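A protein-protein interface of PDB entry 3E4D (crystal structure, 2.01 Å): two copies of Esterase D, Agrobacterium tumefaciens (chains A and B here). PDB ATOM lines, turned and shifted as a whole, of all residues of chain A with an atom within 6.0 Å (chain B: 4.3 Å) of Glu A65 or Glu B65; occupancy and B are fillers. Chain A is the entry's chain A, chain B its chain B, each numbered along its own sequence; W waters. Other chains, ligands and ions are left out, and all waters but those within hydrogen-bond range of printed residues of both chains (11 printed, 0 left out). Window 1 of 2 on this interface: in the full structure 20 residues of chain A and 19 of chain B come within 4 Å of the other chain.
The side-chain carboxylate of Glu A65 is in salt-bridge range of the guanidinium group of Arg B67, at 3.7 Å. The side-chain carboxylate of Glu B65 lies within salt-bridge range of the guanidinium group of Arg A67, at 3.7 Å. N of Phe B11 is in hydrogen-bond range of OG1 of Thr A264 (2.9 Å).
The backbone carbonyl oxygen (O) of Met A61 lies within hydrogen-bond range of the guanidinium group (NH1) of Arg A67 (2.7 Å).
Phe A11 touches Glu B65. Ser B263 touches Phe A11. CA of Lys B63 touches O of Glu A62, at 3.7 Å. OE1 of Glu A65 touches CE2 of Phe B11, 3.7 Å away. Glu A65 touches Glu B65. Phe B11 touches Ser A263.
Glu A65 touches just these residues of chain B: Phe B11, Glu B65 and Arg B67. Of chain A, only Phe A11, Glu A65 and Arg A67 come within 4 Å of Glu B65. Of the printed residues of chain A, Lys B63 touches Glu A62. Of the printed residues of chain B, Arg A67 touches Glu B65 (3.7 Å). Of the printed residues of chain A, Ser B263 touches Phe A11. Of the printed residues of chain B, Phe A11 touches Glu B65 (3.6 Å) and Ser B263 (3.4 Å). The nearest printed residue of chain B that does not touch Glu A65 is Tyr B66 (5.1 Å). The nearest residue of chain A that does not touch Glu B65 is Glu A62 (5.0 Å).
Of the 9 printed residues of chain B, 5 touch a printed residue of chain A. Hydrophobic or aromatic side chains of chain A that line the printed part of chain B: Phe A11. Among the printed residues, Asp or Glu carboxylates within 4 Å of a Lys or Arg side-chain nitrogen of the other chain: Glu A65 with Arg B67 and Arg A67 with Glu B65.
Phe A11 touches Glu B65, and with the chains exchanged Glu A65 touches Phe B11. Phe A11 touches Ser B263, and with the chains exchanged Ser A263 touches Phe B11. Glu B65 touches its own counterpart, Glu A65. Glu A65 touches Arg B67, and with the chains exchanged Arg A67 touches Glu B65. 9 positions are printed for both chains. Of the 9 pairs that touch across the chains among the printed residues, 7 have their exchanged pair printed and touching as well.
Water W10 lies within hydrogen-bond range of OG of Ser B263 (2.6 Å), NE of Arg A67 (2.8 Å) and OE2 of Glu B65 (3.0 Å). Water W11 lies within hydrogen-bond range of OE1 of Glu B65 (2.7 Å), N of Arg A68 (3.0 Å), O of Glu A65 (3.3 Å) and N of Arg A67 (3.4 Å). Water W7 lies within hydrogen-bond range of the guanidinium group (NE) of Arg B67, the side-chain carboxylate (OE2) of Glu A65 and the side-chain hydroxyl (OG) of Ser A263. Water W5 bridges NZ of Lys B63 (2.7 Å) and OE2 of Glu A62 (3.3 Å). Water W6 bridges NH2 of Arg B67 (2.8 Å) and O of Lys A63 (3.2 Å). Water W2 lies within hydrogen-bond range of OE2 of Glu A65 (2.9 Å) and N of Glu B65 (3.1 Å).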
ATOM      1  N   PHE A  11      27.667  22.320   0.576  1.00  0.00           N
ATOM      2  CA  PHE A  11      26.395  21.895  -0.042  1.00  0.00           C
ATOM      3  C   PHE A  11      25.411  23.071  -0.275  1.00  0.00           C
ATOM      4  O   PHE A  11      24.210  22.974   0.002  1.00  0.00           O
ATOM      5  CB  PHE A  11      25.751  20.771   0.789  1.00  0.00           C
ATOM      6  CG  PHE A  11      26.555  19.483   0.810  1.00  0.00           C
ATOM      7  CD1 PHE A  11      26.471  18.578  -0.246  1.00  0.00           C
ATOM      8  CD2 PHE A  11      27.392  19.177   1.884  1.00  0.00           C
ATOM      9  CE1 PHE A  11      27.214  17.379  -0.230  1.00  0.00           C
ATOM     10  CE2 PHE A  11      28.137  17.984   1.902  1.00  0.00           C
ATOM     11  CZ  PHE A  11      28.042  17.089   0.846  1.00  0.00           C
ATOM     12  N   VAL A  60      30.645  16.895  16.063  1.00  0.00           N
ATOM     13  CA  VAL A  60      29.552  16.675  15.111  1.00  0.00           C
ATOM     14  C   VAL A  60      29.695  17.554  13.860  1.00  0.00           C
ATOM     15  O   VAL A  60      29.439  17.106  12.739  1.00  0.00           O
ATOM     16  CB  VAL A  60      28.144  16.839  15.774  1.00  0.00           C
ATOM     17  CG1 VAL A  60      27.907  18.272  16.310  1.00  0.00           C
ATOM     18  CG2 VAL A  60      27.025  16.410  14.799  1.00  0.00           C
ATOM     19  N   MET A  61      30.106  18.809  14.047  1.00  0.00           N
ATOM     20  CA  MET A  61      30.263  19.708  12.912  1.00  0.00           C
ATOM     21  C   MET A  61      31.228  19.107  11.899  1.00  0.00           C
ATOM     22  O   MET A  61      30.987  19.126  10.675  1.00  0.00           O
ATOM     23  CB  MET A  61      30.771  21.068  13.359  1.00  0.00           C
ATOM     24  CG  MET A  61      30.772  22.103  12.236  1.00  0.00           C
ATOM     25  SD  MET A  61      31.565  23.792  12.726  1.00  0.00           S
ATOM     26  CE  MET A  61      33.415  23.203  12.924  1.00  0.00           C
ATOM     27  N   GLU A  62      32.333  18.580  12.408  1.00  0.00           N
ATOM     28  CA  GLU A  62      33.330  17.970  11.548  1.00  0.00           C
ATOM     29  C   GLU A  62      32.960  16.563  11.065  1.00  0.00           C
ATOM     30  O   GLU A  62      33.229  16.212   9.906  1.00  0.00           O
ATOM     31  CB  GLU A  62      34.689  17.970  12.239  1.00  0.00           C
ATOM     32  CG  GLU A  62      35.216  19.362  12.434  1.00  0.00           C
ATOM     33  CD  GLU A  62      36.570  19.414  13.108  1.00  0.00           C
ATOM     34  OE1 GLU A  62      37.051  18.380  13.619  1.00  0.00           O
ATOM     35  OE2 GLU A  62      37.153  20.511  13.105  1.00  0.00           O
ATOM     36  N   LYS A  63      32.299  15.784  11.923  1.00  0.00           N
ATOM     37  CA  LYS A  63      32.141  14.343  11.660  1.00  0.00           C
ATOM     38  C   LYS A  63      30.721  13.780  11.572  1.00  0.00           C
ATOM     39  O   LYS A  63      30.552  12.628  11.207  1.00  0.00           O
ATOM     40  CB  LYS A  63      32.910  13.535  12.703  1.00  0.00           C
ATOM     41  CG  LYS A  63      34.369  13.965  12.875  1.00  0.00           C
ATOM     42  CD  LYS A  63      35.113  13.044  13.826  1.00  0.00           C
ATOM     43  CE  LYS A  63      34.553  13.140  15.231  1.00  0.00           C
ATOM     44  NZ  LYS A  63      35.267  12.195  16.134  1.00  0.00           N
ATOM     45  N   GLY A  64      29.712  14.576  11.913  1.00  0.00           N
ATOM     46  CA  GLY A  64      28.336  14.091  11.938  1.00  0.00           C
ATOM     47  C   GLY A  64      27.734  13.795  10.574  1.00  0.00           C
ATOM     48  O   GLY A  64      26.721  13.095  10.492  1.00  0.00           O
ATOM     49  N   GLU A  65      28.352  14.343   9.525  1.00  0.00           N
ATOM     50  CA  GLU A  65      27.855  14.259   8.124  1.00  0.00           C
ATOM     51  C   GLU A  65      26.379  14.638   7.951  1.00  0.00           C
ATOM     52  O   GLU A  65      25.587  13.897   7.353  1.00  0.00           O
ATOM     53  CB  GLU A  65      28.187  12.886   7.518  1.00  0.00           C
ATOM     54  CG  GLU A  65      29.692  12.603   7.532  1.00  0.00           C
ATOM     55  CD  GLU A  65      30.090  11.330   6.823  1.00  0.00           C
ATOM     56  OE1 GLU A  65      29.272  10.770   6.060  1.00  0.00           O
ATOM     57  OE2 GLU A  65      31.254  10.894   7.016  1.00  0.00           O
ATOM     58  N   TYR A  66      26.024  15.815   8.470  1.00  0.00           N
ATOM     59  CA  TYR A  66      24.638  16.313   8.458  1.00  0.00           C
ATOM     60  C   TYR A  66      24.321  17.372   7.394  1.00  0.00           C
ATOM     61  O   TYR A  66      23.152  17.645   7.140  1.00  0.00           O
ATOM     62  CB  TYR A  66      24.234  16.864   9.856  1.00  0.00           C
ATOM     63  CG  TYR A  66      25.051  18.050  10.350  1.00  0.00           C
ATOM     64  CD1 TYR A  66      25.877  17.933  11.484  1.00  0.00           C
ATOM     65  CD2 TYR A  66      24.977  19.308   9.721  1.00  0.00           C
ATOM     66  CE1 TYR A  66      26.621  19.015  11.942  1.00  0.00           C
ATOM     67  CE2 TYR A  66      25.722  20.399  10.186  1.00  0.00           C
ATOM     68  CZ  TYR A  66      26.549  20.235  11.295  1.00  0.00           C
ATOM     69  OH  TYR A  66      27.297  21.295  11.759  1.00  0.00           O
ATOM     70  N   ARG A  67      25.346  17.977   6.789  1.00  0.00           N
ATOM     71  CA  ARG A  67      25.131  19.119   5.887  1.00  0.00           C
ATOM     72  C   ARG A  67      24.468  18.741   4.552  1.00  0.00           C
ATOM     73  O   ARG A  67      23.629  19.497   4.045  1.00  0.00           O
ATOM     74  CB  ARG A  67      26.430  19.912   5.674  1.00  0.00           C
ATOM     75  CG  ARG A  67      26.808  20.820   6.874  1.00  0.00           C
ATOM     76  CD  ARG A  67      28.142  21.549   6.695  1.00  0.00           C
ATOM     77  NE  ARG A  67      29.262  20.613   6.769  1.00  0.00           N
ATOM     78  CZ  ARG A  67      29.887  20.251   7.897  1.00  0.00           C
ATOM     79  NH1 ARG A  67      29.517  20.767   9.071  1.00  0.00           N
ATOM     80  NH2 ARG A  67      30.893  19.356   7.848  1.00  0.00           N
ATOM     81  N   ARG A  68      24.826  17.585   3.994  1.00  0.00           N
ATOM     82  CA  ARG A  68      24.245  17.145   2.705  1.00  0.00           C
ATOM     83  C   ARG A  68      22.730  17.035   2.781  1.00  0.00           C
ATOM     84  O   ARG A  68      22.024  17.594   1.935  1.00  0.00           O
ATOM     85  CB  ARG A  68      24.825  15.807   2.253  1.00  0.00           C
ATOM     86  CG  ARG A  68      24.332  15.310   0.866  1.00  0.00           C
ATOM     87  CD  ARG A  68      24.937  13.932   0.561  1.00  0.00           C
ATOM     88  NE  ARG A  68      25.181  13.165   1.794  1.00  0.00           N
ATOM     89  CZ  ARG A  68      24.248  12.510   2.491  1.00  0.00           C
ATOM     90  NH1 ARG A  68      22.989  12.503   2.088  1.00  0.00           N
ATOM     91  NH2 ARG A  68      24.579  11.861   3.602  1.00  0.00           N
ATOM     92  N   MET A  69      22.240  16.323   3.800  1.00  0.00           N
ATOM     93  CA  MET A  69      20.806  16.111   3.988  1.00  0.00           C
ATOM     94  C   MET A  69      20.107  17.317   4.611  1.00  0.00           C
ATOM     95  O   MET A  69      18.961  17.597   4.261  1.00  0.00           O
ATOM     96  CB  MET A  69      20.534  14.803   4.738  1.00  0.00           C
ATOM     97  CG  MET A  69      19.106  14.315   4.754  1.00  0.00           C
ATOM     98  SD  MET A  69      18.257  14.114   2.971  1.00  0.00           S
ATOM     99  CE  MET A  69      19.777  13.569   1.902  1.00  0.00           C
ATOM    100  N   SER A 263      27.157   9.170  12.003  1.00  0.00           N
ATOM    101  CA  SER A 263      27.139   9.588  10.610  1.00  0.00           C
ATOM    102  C   SER A 263      26.408   8.608   9.703  1.00  0.00           C
ATOM    103  O   SER A 263      25.719   9.031   8.776  1.00  0.00           O
ATOM    104  CB  SER A 263      28.566   9.845  10.092  1.00  0.00           C
ATOM    105  OG  SER A 263      29.377   8.663  10.116  1.00  0.00           O
ATOM    106  N   THR A 264      26.582   7.307   9.943  1.00  0.00           N
ATOM    107  CA  THR A 264      25.840   6.296   9.202  1.00  0.00           C
ATOM    108  C   THR A 264      24.321   6.504   9.253  1.00  0.00           C
ATOM    109  O   THR A 264      23.651   6.435   8.214  1.00  0.00           O
ATOM    110  CB  THR A 264      26.190   4.864   9.645  1.00  0.00           C
ATOM    111  OG1 THR A 264      27.581   4.649   9.427  1.00  0.00           O
ATOM    112  CG2 THR A 264      25.371   3.826   8.837  1.00  0.00           C
ATOM    113  N   MET A 266      22.724   9.309  10.433  1.00  0.00           N
ATOM    114  CA  MET A 266      22.369  10.742  10.439  1.00  0.00           C
ATOM    115  C   MET A 266      21.218  11.151   9.505  1.00  0.00           C
ATOM    116  O   MET A 266      20.287  11.833   9.951  1.00  0.00           O
ATOM    117  CB  MET A 266      23.621  11.600  10.198  1.00  0.00           C
ATOM    118  CG  MET A 266      23.383  13.121  10.197  1.00  0.00           C
ATOM    119  SD  MET A 266      22.600  13.845  11.826  1.00  0.00           S
ATOM    120  CE  MET A 266      24.144  13.809  13.022  1.00  0.00           C
ATOM    121  N   ASP A 267      21.280  10.742   8.228  1.00  0.00           N
ATOM    122  CA  ASP A 267      20.209  11.017   7.239  1.00  0.00           C
ATOM    123  C   ASP A 267      18.828  10.550   7.707  1.00  0.00           C
ATOM    124  O   ASP A 267      17.843  11.287   7.576  1.00  0.00           O
ATOM    125  CB  ASP A 267      20.532  10.379   5.877  1.00  0.00           C
ATOM    126  CG  ASP A 267      21.590  11.143   5.089  1.00  0.00           C
ATOM    127  OD1 ASP A 267      22.235  12.063   5.635  1.00  0.00           O
ATOM    128  OD2 ASP A 267      21.777  10.821   3.892  1.00  0.00           O
ATOM    129  N   LEU A 270      17.680  13.118  10.254  1.00  0.00           N
ATOM    130  CA  LEU A 270      17.333  14.383   9.632  1.00  0.00           C
ATOM    131  C   LEU A 270      15.961  14.298   8.943  1.00  0.00           C
ATOM    132  O   LEU A 270      15.148  15.227   9.049  1.00  0.00           O
ATOM    133  CB  LEU A 270      18.455  14.838   8.682  1.00  0.00           C
ATOM    134  CG  LEU A 270      19.753  15.269   9.390  1.00  0.00           C
ATOM    135  CD1 LEU A 270      20.879  15.495   8.397  1.00  0.00           C
ATOM    136  CD2 LEU A 270      19.534  16.533  10.257  1.00  0.00           C
ATOM    137  N   PHE B  11      28.750   2.878   7.467  1.00  0.00           N
ATOM    138  CA  PHE B  11      27.999   2.506   6.254  1.00  0.00           C
ATOM    139  C   PHE B  11      28.213   1.045   5.799  1.00  0.00           C
ATOM    140  O   PHE B  11      28.402   0.769   4.606  1.00  0.00           O
ATOM    141  CB  PHE B  11      28.302   3.471   5.107  1.00  0.00           C
ATOM    142  CG  PHE B  11      27.845   4.884   5.359  1.00  0.00           C
ATOM    143  CD1 PHE B  11      26.536   5.272   5.073  1.00  0.00           C
ATOM    144  CD2 PHE B  11      28.724   5.832   5.877  1.00  0.00           C
ATOM    145  CE1 PHE B  11      26.111   6.591   5.298  1.00  0.00           C
ATOM    146  CE2 PHE B  11      28.299   7.149   6.104  1.00  0.00           C
ATOM    147  CZ  PHE B  11      26.995   7.518   5.813  1.00  0.00           C
ATOM    148  N   LYS B  63      36.602  14.234   7.967  1.00  0.00           N
ATOM    149  CA  LYS B  63      35.821  15.320   7.369  1.00  0.00           C
ATOM    150  C   LYS B  63      35.541  15.227   5.852  1.00  0.00           C
ATOM    151  O   LYS B  63      34.782  16.039   5.334  1.00  0.00           O
ATOM    152  CB  LYS B  63      36.488  16.668   7.655  1.00  0.00           C
ATOM    153  CG  LYS B  63      36.865  16.938   9.152  1.00  0.00           C
ATOM    154  CD  LYS B  63      37.402  18.361   9.335  1.00  0.00           C
ATOM    155  CE  LYS B  63      38.692  18.590   8.539  1.00  0.00           C
ATOM    156  NZ  LYS B  63      39.282  19.926   8.802  1.00  0.00           N
ATOM    157  N   GLY B  64      36.150  14.274   5.152  1.00  0.00           N
ATOM    158  CA  GLY B  64      35.998  14.194   3.689  1.00  0.00           C
ATOM    159  C   GLY B  64      34.637  13.707   3.195  1.00  0.00           C
ATOM    160  O   GLY B  64      34.276  13.912   2.016  1.00  0.00           O
ATOM    161  N   GLU B  65      33.894  13.058   4.091  1.00  0.00           N
ATOM    162  CA  GLU B  65      32.583  12.461   3.785  1.00  0.00           C
ATOM    163  C   GLU B  65      32.629  11.562   2.528  1.00  0.00           C
ATOM    164  O   GLU B  65      31.814  11.698   1.606  1.00  0.00           O
ATOM    165  CB  GLU B  65      31.493  13.550   3.701  1.00  0.00           C
ATOM    166  CG  GLU B  65      31.554  14.557   4.872  1.00  0.00           C
ATOM    167  CD  GLU B  65      30.358  15.489   4.945  1.00  0.00           C
ATOM    168  OE1 GLU B  65      29.481  15.438   4.062  1.00  0.00           O
ATOM    169  OE2 GLU B  65      30.287  16.275   5.914  1.00  0.00           O
ATOM    170  N   TYR B  66      33.589  10.635   2.514  1.00  0.00           N
ATOM    171  CA  TYR B  66      33.746   9.686   1.404  1.00  0.00           C
ATOM    172  C   TYR B  66      33.122   8.309   1.634  1.00  0.00           C
ATOM    173  O   TYR B  66      32.915   7.568   0.667  1.00  0.00           O
ATOM    174  CB  TYR B  66      35.228   9.501   1.024  1.00  0.00           C
ATOM    175  CG  TYR B  66      36.119   8.976   2.143  1.00  0.00           C
ATOM    176  CD1 TYR B  66      37.033   9.827   2.795  1.00  0.00           C
ATOM    177  CD2 TYR B  66      36.072   7.628   2.536  1.00  0.00           C
ATOM    178  CE1 TYR B  66      37.864   9.355   3.800  1.00  0.00           C
ATOM    179  CE2 TYR B  66      36.899   7.147   3.566  1.00  0.00           C
ATOM    180  CZ  TYR B  66      37.796   8.018   4.184  1.00  0.00           C
ATOM    181  OH  TYR B  66      38.619   7.562   5.193  1.00  0.00           O
ATOM    182  N   ARG B  67      32.837   7.965   2.895  1.00  0.00           N
ATOM    183  CA  ARG B  67      32.418   6.594   3.235  1.00  0.00           C
ATOM    184  C   ARG B  67      31.059   6.164   2.676  1.00  0.00           C
ATOM    185  O   ARG B  67      30.915   5.009   2.301  1.00  0.00           O
ATOM    186  CB  ARG B  67      32.484   6.327   4.748  1.00  0.00           C
ATOM    187  CG  ARG B  67      33.906   6.117   5.285  1.00  0.00           C
ATOM    188  CD  ARG B  67      33.920   5.824   6.792  1.00  0.00           C
ATOM    189  NE  ARG B  67      33.613   7.030   7.558  1.00  0.00           N
ATOM    190  CZ  ARG B  67      34.508   7.981   7.814  1.00  0.00           C
ATOM    191  NH1 ARG B  67      35.762   7.855   7.382  1.00  0.00           N
ATOM    192  NH2 ARG B  67      34.149   9.066   8.480  1.00  0.00           N
ATOM    193  N   SER B 263      34.309  17.977   0.859  1.00  0.00           N
ATOM    194  CA  SER B 263      33.148  17.122   1.105  1.00  0.00           C
ATOM    195  C   SER B 263      31.951  17.367   0.168  1.00  0.00           C
ATOM    196  O   SER B 263      31.244  16.414  -0.185  1.00  0.00           O
ATOM    197  CB  SER B 263      32.677  17.231   2.571  1.00  0.00           C
ATOM    198  OG  SER B 263      32.214  18.539   2.873  1.00  0.00           O
ATOM    199  N   MET B 266      33.010  15.580  -3.032  1.00  0.00           N
ATOM    200  CA  MET B 266      33.507  14.221  -2.856  1.00  0.00           C
ATOM    201  C   MET B 266      32.751  13.147  -3.661  1.00  0.00           C
ATOM    202  O   MET B 266      33.400  12.307  -4.300  1.00  0.00           O
ATOM    203  CB  MET B 266      33.554  13.849  -1.358  1.00  0.00           C
ATOM    204  CG  MET B 266      34.092  12.458  -1.085  1.00  0.00           C
ATOM    205  SD  MET B 266      35.897  12.177  -1.774  1.00  0.00           S
ATOM    206  CE  MET B 266      36.906  13.192  -0.422  1.00  0.00           C
ATOM    207  N   ASP B 267      31.416  13.150  -3.630  1.00  0.00           N
ATOM    208  CA  ASP B 267      30.641  12.145  -4.378  1.00  0.00           C
ATOM    209  C   ASP B 267      30.952  12.173  -5.889  1.00  0.00           C
ATOM    210  O   ASP B 267      31.086  11.117  -6.513  1.00  0.00           O
ATOM    211  CB  ASP B 267      29.125  12.272  -4.159  1.00  0.00           C
ATOM    212  CG  ASP B 267      28.675  11.812  -2.778  1.00  0.00           C
ATOM    213  OD1 ASP B 267      29.523  11.538  -1.908  1.00  0.00           O
ATOM    214  OD2 ASP B 267      27.447  11.730  -2.563  1.00  0.00           O
HETATM  215  O   HOH W   1      30.906  15.878   8.632  1.00  0.00           O
HETATM  216  O   HOH W   2      33.631  12.529   7.086  1.00  0.00           O
HETATM  217  O   HOH W   3      28.050  13.436   2.566  1.00  0.00           O
HETATM  218  O   HOH W   4      30.216   9.877   3.720  1.00  0.00           O
HETATM  219  O   HOH W   5      39.857  19.735  11.473  1.00  0.00           O
HETATM  220  O   HOH W   6      33.063  11.032  10.166  1.00  0.00           O
HETATM  221  O   HOH W   7      31.254   8.332   7.946  1.00  0.00           O
HETATM  222  O   HOH W   8      32.913   9.479   5.407  1.00  0.00           O
HETATM  223  O   HOH W   9      28.243  17.619   7.073  1.00  0.00           O
HETATM  224  O   HOH W  10      30.424  19.000   4.744  1.00  0.00           O
HETATM  225  O   HOH W  11      26.901  15.664   4.856  1.00  0.00           O
